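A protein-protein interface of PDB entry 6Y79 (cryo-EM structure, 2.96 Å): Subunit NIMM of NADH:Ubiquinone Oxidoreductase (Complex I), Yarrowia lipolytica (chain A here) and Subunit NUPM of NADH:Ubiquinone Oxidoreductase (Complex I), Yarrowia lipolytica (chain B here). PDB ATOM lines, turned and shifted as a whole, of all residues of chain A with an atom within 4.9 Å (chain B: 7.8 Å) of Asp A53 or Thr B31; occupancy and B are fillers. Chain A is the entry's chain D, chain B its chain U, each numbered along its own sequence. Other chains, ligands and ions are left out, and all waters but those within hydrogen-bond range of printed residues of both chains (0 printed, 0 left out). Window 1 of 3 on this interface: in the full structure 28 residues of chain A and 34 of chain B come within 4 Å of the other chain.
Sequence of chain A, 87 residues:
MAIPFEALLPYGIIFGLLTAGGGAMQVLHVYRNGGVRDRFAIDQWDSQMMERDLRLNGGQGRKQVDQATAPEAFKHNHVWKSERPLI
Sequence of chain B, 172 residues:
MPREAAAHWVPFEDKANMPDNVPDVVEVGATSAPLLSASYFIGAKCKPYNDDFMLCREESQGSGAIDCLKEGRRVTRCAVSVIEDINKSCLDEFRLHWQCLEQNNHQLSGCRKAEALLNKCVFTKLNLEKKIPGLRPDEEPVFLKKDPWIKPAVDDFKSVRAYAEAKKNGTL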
ATOM      1  N   MET A  49     -18.351 -16.273 -11.822  1.00  0.00           N
ATOM      2  CA  MET A  49     -19.298 -15.793 -10.822  1.00  0.00           C
ATOM      3  C   MET A  49     -18.975 -16.344  -9.435  1.00  0.00           C
ATOM      4  O   MET A  49     -19.089 -15.630  -8.427  1.00  0.00           O
ATOM      5  CB  MET A  49     -20.717 -16.159 -11.237  1.00  0.00           C
ATOM      6  CG  MET A  49     -21.708 -15.398 -10.476  1.00  0.00           C
ATOM      7  SD  MET A  49     -21.574 -13.618 -10.654  1.00  0.00           S
ATOM      8  CE  MET A  49     -22.371 -13.457 -12.228  1.00  0.00           C
ATOM      9  N   MET A  50     -18.511 -17.595  -9.372  1.00  0.00           N
ATOM     10  CA  MET A  50     -18.088 -18.190  -8.109  1.00  0.00           C
ATOM     11  C   MET A  50     -16.849 -17.506  -7.541  1.00  0.00           C
ATOM     12  O   MET A  50     -16.763 -17.296  -6.328  1.00  0.00           O
ATOM     13  CB  MET A  50     -17.828 -19.681  -8.288  1.00  0.00           C
ATOM     14  CG  MET A  50     -19.077 -20.510  -8.377  1.00  0.00           C
ATOM     15  SD  MET A  50     -18.701 -22.221  -8.768  1.00  0.00           S
ATOM     16  CE  MET A  50     -18.192 -22.811  -7.161  1.00  0.00           C
ATOM     17  N   GLU A  51     -15.867 -17.170  -8.385  1.00  0.00           N
ATOM     18  CA  GLU A  51     -14.704 -16.449  -7.859  1.00  0.00           C
ATOM     19  C   GLU A  51     -15.067 -15.024  -7.449  1.00  0.00           C
ATOM     20  O   GLU A  51     -14.503 -14.495  -6.480  1.00  0.00           O
ATOM     21  CB  GLU A  51     -13.548 -16.467  -8.859  1.00  0.00           C
ATOM     22  CG  GLU A  51     -13.814 -15.643 -10.068  1.00  0.00           C
ATOM     23  CD  GLU A  51     -12.852 -15.784 -11.187  1.00  0.00           C
ATOM     24  OE1 GLU A  51     -11.847 -16.548 -11.131  1.00  0.00           O
ATOM     25  OE2 GLU A  51     -13.156 -15.173 -12.262  1.00  0.00           O
ATOM     26  N   ARG A  52     -16.066 -14.417  -8.109  1.00  0.00           N
ATOM     27  CA  ARG A  52     -16.504 -13.088  -7.685  1.00  0.00           C
ATOM     28  C   ARG A  52     -17.203 -13.135  -6.332  1.00  0.00           C
ATOM     29  O   ARG A  52     -17.031 -12.244  -5.490  1.00  0.00           O
ATOM     30  CB  ARG A  52     -17.429 -12.483  -8.736  1.00  0.00           C
ATOM     31  CG  ARG A  52     -17.873 -11.098  -8.414  1.00  0.00           C
ATOM     32  CD  ARG A  52     -18.818 -10.574  -9.444  1.00  0.00           C
ATOM     33  NE  ARG A  52     -19.251  -9.232  -9.092  1.00  0.00           N
ATOM     34  CZ  ARG A  52     -20.292  -8.968  -8.316  1.00  0.00           C
ATOM     35  NH1 ARG A  52     -21.018  -9.954  -7.811  1.00  0.00           N
ATOM     36  NH2 ARG A  52     -20.607  -7.713  -8.049  1.00  0.00           N
ATOM     37  N   ASP A  53     -17.966 -14.191  -6.086  1.00  0.00           N
ATOM     38  CA  ASP A  53     -18.662 -14.275  -4.809  1.00  0.00           C
ATOM     39  C   ASP A  53     -17.730 -14.684  -3.677  1.00  0.00           C
ATOM     40  O   ASP A  53     -17.945 -14.276  -2.531  1.00  0.00           O
ATOM     41  CB  ASP A  53     -19.837 -15.226  -4.917  1.00  0.00           C
ATOM     42  CG  ASP A  53     -20.821 -14.785  -5.956  1.00  0.00           C
ATOM     43  OD1 ASP A  53     -20.703 -13.653  -6.482  1.00  0.00           O
ATOM     44  OD2 ASP A  53     -21.708 -15.586  -6.252  1.00  0.00           O
ATOM     45  N   LEU A  54     -16.680 -15.465  -3.972  1.00  0.00           N
ATOM     46  CA  LEU A  54     -15.631 -15.673  -2.975  1.00  0.00           C
ATOM     47  C   LEU A  54     -14.912 -14.371  -2.661  1.00  0.00           C
ATOM     48  O   LEU A  54     -14.482 -14.159  -1.523  1.00  0.00           O
ATOM     49  CB  LEU A  54     -14.633 -16.730  -3.459  1.00  0.00           C
ATOM     50  CG  LEU A  54     -13.509 -17.304  -2.586  1.00  0.00           C
ATOM     51  CD1 LEU A  54     -13.192 -18.698  -3.080  1.00  0.00           C
ATOM     52  CD2 LEU A  54     -12.220 -16.498  -2.558  1.00  0.00           C
ATOM     53  N   ARG A  55     -14.773 -13.493  -3.654  1.00  0.00           N
ATOM     54  CA  ARG A  55     -14.195 -12.181  -3.394  1.00  0.00           C
ATOM     55  C   ARG A  55     -15.110 -11.311  -2.548  1.00  0.00           C
ATOM     56  O   ARG A  55     -14.631 -10.540  -1.712  1.00  0.00           O
ATOM     57  CB  ARG A  55     -13.889 -11.489  -4.723  1.00  0.00           C
ATOM     58  CG  ARG A  55     -13.081 -10.228  -4.624  1.00  0.00           C
ATOM     59  CD  ARG A  55     -12.423  -9.928  -5.945  1.00  0.00           C
ATOM     60  NE  ARG A  55     -13.361 -10.021  -7.054  1.00  0.00           N
ATOM     61  CZ  ARG A  55     -13.965  -8.976  -7.608  1.00  0.00           C
ATOM     62  NH1 ARG A  55     -13.731  -7.757  -7.147  1.00  0.00           N
ATOM     63  NH2 ARG A  55     -14.802  -9.150  -8.619  1.00  0.00           N
ATOM     64  N   LEU A  56     -16.420 -11.435  -2.736  1.00  0.00           N
ATOM     65  CA  LEU A  56     -17.342 -10.499  -2.106  1.00  0.00           C
ATOM     66  C   LEU A  56     -17.722 -10.930  -0.694  1.00  0.00           C
ATOM     67  O   LEU A  56     -17.892 -10.083   0.186  1.00  0.00           O
ATOM     68  CB  LEU A  56     -18.581 -10.338  -2.977  1.00  0.00           C
ATOM     69  CG  LEU A  56     -19.703  -9.406  -2.551  1.00  0.00           C
ATOM     70  CD1 LEU A  56     -19.202  -8.035  -2.147  1.00  0.00           C
ATOM     71  CD2 LEU A  56     -20.600  -9.303  -3.747  1.00  0.00           C
ATOM     72  N   ASN A  57     -17.892 -12.236  -0.455  1.00  0.00           N
ATOM     73  CA  ASN A  57     -18.414 -12.665   0.840  1.00  0.00           C
ATOM     74  C   ASN A  57     -17.374 -12.541   1.938  1.00  0.00           C
ATOM     75  O   ASN A  57     -17.719 -12.250   3.085  1.00  0.00           O
ATOM     76  CB  ASN A  57     -18.973 -14.100   0.777  1.00  0.00           C
ATOM     77  CG  ASN A  57     -17.930 -15.161   0.403  1.00  0.00           C
ATOM     78  OD1 ASN A  57     -16.762 -14.877   0.151  1.00  0.00           O
ATOM     79  ND2 ASN A  57     -18.374 -16.404   0.353  1.00  0.00           N
ATOM     80  N   GLY A  58     -16.110 -12.724   1.599  1.00  0.00           N
ATOM     81  CA  GLY A  58     -15.060 -12.707   2.578  1.00  0.00           C
ATOM     82  C   GLY A  58     -14.671 -14.122   2.927  1.00  0.00           C
ATOM     83  O   GLY A  58     -15.306 -14.746   3.781  1.00  0.00           O
ATOM     84  N   GLN A  64     -22.764 -16.488   0.391  1.00  0.00           N
ATOM     85  CA  GLN A  64     -23.821 -15.810  -0.357  1.00  0.00           C
ATOM     86  C   GLN A  64     -24.450 -14.686   0.474  1.00  0.00           C
ATOM     87  O   GLN A  64     -25.578 -14.747   0.967  1.00  0.00           O
ATOM     88  CB  GLN A  64     -24.841 -16.829  -0.864  1.00  0.00           C
ATOM     89  CG  GLN A  64     -24.253 -17.856  -1.810  1.00  0.00           C
ATOM     90  CD  GLN A  64     -24.218 -17.365  -3.219  1.00  0.00           C
ATOM     91  OE1 GLN A  64     -25.116 -16.647  -3.617  1.00  0.00           O
ATOM     92  NE2 GLN A  64     -23.212 -17.764  -3.988  1.00  0.00           N
ATOM     93  N   VAL A  65     -23.606 -13.685   0.682  1.00  0.00           N
ATOM     94  CA  VAL A  65     -24.033 -12.414   1.225  1.00  0.00           C
ATOM     95  C   VAL A  65     -25.045 -11.754   0.299  1.00  0.00           C
ATOM     96  O   VAL A  65     -24.988 -11.869  -0.927  1.00  0.00           O
ATOM     97  CB  VAL A  65     -22.798 -11.529   1.449  1.00  0.00           C
ATOM     98  CG1 VAL A  65     -23.130 -10.250   2.165  1.00  0.00           C
ATOM     99  CG2 VAL A  65     -21.809 -12.301   2.276  1.00  0.00           C
ATOM    100  N   VAL B  28     -21.870  -2.905  -6.088  1.00  0.00           N
ATOM    101  CA  VAL B  28     -22.899  -3.908  -5.848  1.00  0.00           C
ATOM    102  C   VAL B  28     -22.324  -4.974  -4.934  1.00  0.00           C
ATOM    103  O   VAL B  28     -21.269  -5.550  -5.219  1.00  0.00           O
ATOM    104  CB  VAL B  28     -23.403  -4.512  -7.165  1.00  0.00           C
ATOM    105  CG1 VAL B  28     -24.370  -5.654  -6.892  1.00  0.00           C
ATOM    106  CG2 VAL B  28     -24.095  -3.454  -7.969  1.00  0.00           C
ATOM    107  N   GLY B  29     -22.997  -5.209  -3.815  1.00  0.00           N
ATOM    108  CA  GLY B  29     -22.596  -6.206  -2.853  1.00  0.00           C
ATOM    109  C   GLY B  29     -23.434  -7.461  -2.857  1.00  0.00           C
ATOM    110  O   GLY B  29     -23.317  -8.264  -1.926  1.00  0.00           O
ATOM    111  N   ALA B  30     -24.269  -7.665  -3.867  1.00  0.00           N
ATOM    112  CA  ALA B  30     -25.031  -8.893  -3.970  1.00  0.00           C
ATOM    113  C   ALA B  30     -24.214  -9.962  -4.678  1.00  0.00           C
ATOM    114  O   ALA B  30     -23.476  -9.686  -5.628  1.00  0.00           O
ATOM    115  CB  ALA B  30     -26.339  -8.650  -4.718  1.00  0.00           C
ATOM    116  N   THR B  31     -24.369 -11.197  -4.218  1.00  0.00           N
ATOM    117  CA  THR B  31     -23.711 -12.350  -4.813  1.00  0.00           C
ATOM    118  C   THR B  31     -24.667 -12.977  -5.831  1.00  0.00           C
ATOM    119  O   THR B  31     -25.715 -12.407  -6.126  1.00  0.00           O
ATOM    120  CB  THR B  31     -23.277 -13.319  -3.718  1.00  0.00           C
ATOM    121  OG1 THR B  31     -24.427 -13.732  -2.973  1.00  0.00           O
ATOM    122  CG2 THR B  31     -22.314 -12.626  -2.774  1.00  0.00           C
ATOM    123  N   SER B  32     -24.323 -14.163  -6.364  1.00  0.00           N
ATOM    124  CA  SER B  32     -24.950 -14.701  -7.580  1.00  0.00           C
ATOM    125  C   SER B  32     -26.407 -15.072  -7.398  1.00  0.00           C
ATOM    126  O   SER B  32     -27.196 -14.936  -8.334  1.00  0.00           O
ATOM    127  CB  SER B  32     -24.228 -15.950  -8.070  1.00  0.00           C
ATOM    128  OG  SER B  32     -24.288 -17.015  -7.140  1.00  0.00           O
ATOM    129  N   ALA B  33     -26.762 -15.654  -6.259  1.00  0.00           N
ATOM    130  CA  ALA B  33     -28.169 -15.990  -6.054  1.00  0.00           C
ATOM    131  C   ALA B  33     -29.038 -14.747  -5.847  1.00  0.00           C
ATOM    132  O   ALA B  33     -30.131 -14.692  -6.443  1.00  0.00           O
ATOM    133  CB  ALA B  33     -28.294 -17.021  -4.932  1.00  0.00           C
ATOM    134  N   PRO B  34     -28.634 -13.715  -5.079  1.00  0.00           N
ATOM    135  CA  PRO B  34     -29.434 -12.479  -5.113  1.00  0.00           C
ATOM    136  C   PRO B  34     -29.343 -11.708  -6.419  1.00  0.00           C
ATOM    137  O   PRO B  34     -30.294 -11.001  -6.765  1.00  0.00           O
ATOM    138  CB  PRO B  34     -28.875 -11.664  -3.943  1.00  0.00           C
ATOM    139  CG  PRO B  34     -28.307 -12.650  -3.048  1.00  0.00           C
ATOM    140  CD  PRO B  34     -27.707 -13.664  -3.923  1.00  0.00           C
ATOM    141  N   LEU B  35     -28.233 -11.810  -7.149  1.00  0.00           N
ATOM    142  CA  LEU B  35     -28.106 -11.122  -8.430  1.00  0.00           C
ATOM    143  C   LEU B  35     -28.957 -11.790  -9.501  1.00  0.00           C
ATOM    144  O   LEU B  35     -29.598 -11.112 -10.308  1.00  0.00           O
ATOM    145  CB  LEU B  35     -26.640 -11.102  -8.854  1.00  0.00           C
ATOM    146  CG  LEU B  35     -26.020 -10.065  -9.774  1.00  0.00           C
ATOM    147  CD1 LEU B  35     -26.335  -8.665  -9.309  1.00  0.00           C
ATOM    148  CD2 LEU B  35     -24.524 -10.295  -9.803  1.00  0.00           C
ATOM    149  N   LEU B  36     -28.969 -13.120  -9.508  1.00  0.00           N
ATOM    150  CA  LEU B  36     -29.782 -13.895 -10.430  1.00  0.00           C
ATOM    151  C   LEU B  36     -31.254 -13.804 -10.078  1.00  0.00           C
ATOM    152  O   LEU B  36     -32.113 -13.908 -10.961  1.00  0.00           O
ATOM    153  CB  LEU B  36     -29.319 -15.347 -10.403  1.00  0.00           C
ATOM    154  CG  LEU B  36     -29.925 -16.336 -11.385  1.00  0.00           C
ATOM    155  CD1 LEU B  36     -29.660 -15.868 -12.796  1.00  0.00           C
ATOM    156  CD2 LEU B  36     -29.346 -17.712 -11.152  1.00  0.00           C
ATOM    157  N   SER B  37     -31.555 -13.618  -8.796  1.00  0.00           N
ATOM    158  CA  SER B  37     -32.931 -13.445  -8.361  1.00  0.00           C
ATOM    159  C   SER B  37     -33.522 -12.153  -8.895  1.00  0.00           C
ATOM    160  O   SER B  37     -34.616 -12.146  -9.470  1.00  0.00           O
ATOM    161  CB  SER B  37     -32.971 -13.468  -6.843  1.00  0.00           C
ATOM    162  OG  SER B  37     -32.846 -14.795  -6.389  1.00  0.00           O
ATOM    163  N   ALA B  38     -32.806 -11.051  -8.723  1.00  0.00           N
ATOM    164  CA  ALA B  38     -33.309  -9.743  -9.094  1.00  0.00           C
ATOM    165  C   ALA B  38     -32.826  -9.293 -10.455  1.00  0.00           C
ATOM    166  O   ALA B  38     -32.908  -8.103 -10.750  1.00  0.00           O
ATOM    167  CB  ALA B  38     -32.908  -8.717  -8.044  1.00  0.00           C
ATOM    168  N   PHE B  94     -37.704 -12.281  -1.048  1.00  0.00           N
ATOM    169  CA  PHE B  94     -36.510 -12.239  -1.863  1.00  0.00           C
ATOM    170  C   PHE B  94     -35.483 -13.209  -1.317  1.00  0.00           C
ATOM    171  O   PHE B  94     -34.900 -13.994  -2.073  1.00  0.00           O
ATOM    172  CB  PHE B  94     -35.959 -10.822  -1.901  1.00  0.00           C
ATOM    173  CG  PHE B  94     -34.730 -10.684  -2.735  1.00  0.00           C
ATOM    174  CD1 PHE B  94     -34.803 -10.740  -4.110  1.00  0.00           C
ATOM    175  CD2 PHE B  94     -33.496 -10.496  -2.142  1.00  0.00           C
ATOM    176  CE1 PHE B  94     -33.678 -10.610  -4.878  1.00  0.00           C
ATOM    177  CE2 PHE B  94     -32.364 -10.370  -2.912  1.00  0.00           C
ATOM    178  CZ  PHE B  94     -32.456 -10.429  -4.280  1.00  0.00           C
ATOM    179  N   TRP B  98     -33.789 -16.513  -3.235  1.00  0.00           N
ATOM    180  CA  TRP B  98     -32.388 -16.836  -3.514  1.00  0.00           C
ATOM    181  C   TRP B  98     -31.820 -17.899  -2.578  1.00  0.00           C
ATOM    182  O   TRP B  98     -30.830 -18.552  -2.938  1.00  0.00           O
ATOM    183  CB  TRP B  98     -31.497 -15.582  -3.519  1.00  0.00           C
ATOM    184  CG  TRP B  98     -31.330 -14.800  -2.274  1.00  0.00           C
ATOM    185  CD1 TRP B  98     -31.964 -13.653  -1.953  1.00  0.00           C
ATOM    186  CD2 TRP B  98     -30.401 -15.049  -1.222  1.00  0.00           C
ATOM    187  NE1 TRP B  98     -31.537 -13.190  -0.743  1.00  0.00           N
ATOM    188  CE2 TRP B  98     -30.568 -14.030  -0.273  1.00  0.00           C
ATOM    189  CE3 TRP B  98     -29.453 -16.043  -0.981  1.00  0.00           C
ATOM    190  CZ2 TRP B  98     -29.830 -13.976   0.898  1.00  0.00           C
ATOM    191  CZ3 TRP B  98     -28.722 -15.988   0.178  1.00  0.00           C
ATOM    192  CH2 TRP B  98     -28.912 -14.962   1.104  1.00  0.00           C
ATOM    193  N   GLU B 102     -29.792 -21.111  -4.184  1.00  0.00           N
ATOM    194  CA  GLU B 102     -28.429 -21.577  -3.935  1.00  0.00           C
ATOM    195  C   GLU B 102     -28.334 -23.086  -3.831  1.00  0.00           C
ATOM    196  O   GLU B 102     -27.251 -23.652  -4.006  1.00  0.00           O
ATOM    197  CB  GLU B 102     -27.867 -20.938  -2.697  1.00  0.00           C
ATOM    198  CG  GLU B 102     -28.435 -21.200  -1.356  1.00  0.00           C
ATOM    199  CD  GLU B 102     -27.712 -20.299  -0.332  1.00  0.00           C
ATOM    200  OE1 GLU B 102     -26.855 -19.538  -0.817  1.00  0.00           O
ATOM    201  OE2 GLU B 102     -27.998 -20.373   0.843  1.00  0.00           O
ATOM    202  N   HIS B 106     -28.309 -23.135  -9.024  1.00  0.00           N
ATOM    203  CA  HIS B 106     -28.835 -21.829  -9.449  1.00  0.00           C
ATOM    204  C   HIS B 106     -29.752 -21.939 -10.659  1.00  0.00           C
ATOM    205  O   HIS B 106     -29.833 -21.024 -11.475  1.00  0.00           O
ATOM    206  CB  HIS B 106     -27.717 -20.810  -9.689  1.00  0.00           C
ATOM    207  CG  HIS B 106     -27.048 -20.343  -8.435  1.00  0.00           C
ATOM    208  ND1 HIS B 106     -26.155 -21.122  -7.736  1.00  0.00           N
ATOM    209  CD2 HIS B 106     -27.141 -19.180  -7.751  1.00  0.00           C
ATOM    210  CE1 HIS B 106     -25.716 -20.458  -6.684  1.00  0.00           C
ATOM    211  NE2 HIS B 106     -26.305 -19.277  -6.665  1.00  0.00           N
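Printed residues of chain B within 4 Å of Met A49: Ser B32. Printed residues of chain B within 4 Å of Arg A52: Val B28 (3.6 Å) and Ala B30 (3.3 Å). Asp A53 touches two residues of chain B. Printed residues of chain A within 4 Å of Val B28: Arg A52 (3.6 Å). Of the printed residues of chain A, Ala B30 touches Arg A52 and Leu A56. Of the printed residues of chain A, Pro B34 touches Gln A64 (3.96 Å). Leu B36 touches none of the printed residues of chain A. The nearest residue of chain B that does not touch Asp A53 is Ala B30 (4.9 Å). The nearest residue of chain A that does not touch Thr B31 is Arg A52 (4.7 Å). The nearest printed residue of chain B that does not touch Val A65 is Pro B34 (4.02 Å).
Ser B32 touches Met A49 (CB to CG, 3.5 Å). Arg A52 touches Val B28 (NH2 to O, 3.6 Å). Thr B31 touches Asp A53 (CB to CG, 3.6 Å). Leu A56 touches Gly B29. Leu A56 touches Ala B30 (CD2 to O, 3.5 Å). Thr B31 touches Leu A56. Pro B34 touches Gln A64 (CD to OE1, 3.96 Å). Trp B98 touches Gln A64 (CH2 to O, 3.3 Å). Gln A64 touches Glu B102 (CG to OE1, 3.3 Å).
A ring nitrogen (NE2) of His B106 lies within hydrogen-bond range of the side-chain hydroxyl of Ser B32 (3.1 Å). The side-chain hydroxyl of Ser B37 lies within hydrogen-bond range of the backbone carbonyl oxygen of Ala B33 (2.7 Å). NH1 of Arg A52 is in salt-bridge range of OD1 of Asp A53 (3.9 Å). The backbone carbonyl oxygen (O) of Asp A53 lies close to the side-chain amide oxygen (OD1) of Asn A57, 3.0 Å away. The side-chain carboxylate of Asp A53 sits at hydrogen-bond distance from the side-chain amide nitrogen of Gln A64, 3.5 Å away.
Printed residues of chain B that touch a printed residue of chain A: Val B28, Gly B29, Ala B30, Thr B31, Ser B32, Ala B33, Pro B34, Trp B98 and Glu B102. Along chain B the printed residues that touch a printed residue of chain A span positions 28 to 102. Of the 12 printed residues of chain A, 6 touch a printed residue of chain B. Hydrophobic or aromatic side chains of chain A within 4 Å of the printed part of chain B: Met A49 and Leu A56.
NH1 of Arg A52 lies within hydrogen-bond range of O of Ala B30 (3.3 Å). The side-chain amide oxygen (OE1) of Gln A64 lies within hydrogen-bond range of the side-chain hydroxyl (OG1) of Thr B31, at 3.1 Å. OG1 of Thr B31 lies within hydrogen-bond range of O of Val A65, at 2.8 Å. N of Ser B32 sits at hydrogen-bond distance from OD2 of Asp A53, 3.0 Å away. The side-chain hydroxyl (OG) of Ser B32 is in hydrogen-bond range of the side-chain amide nitrogen (NE2) of Gln A64 (3.4 Å). OE1 of Gln A64 sits at hydrogen-bond distance from N of Ala B33 (3.3 Å).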
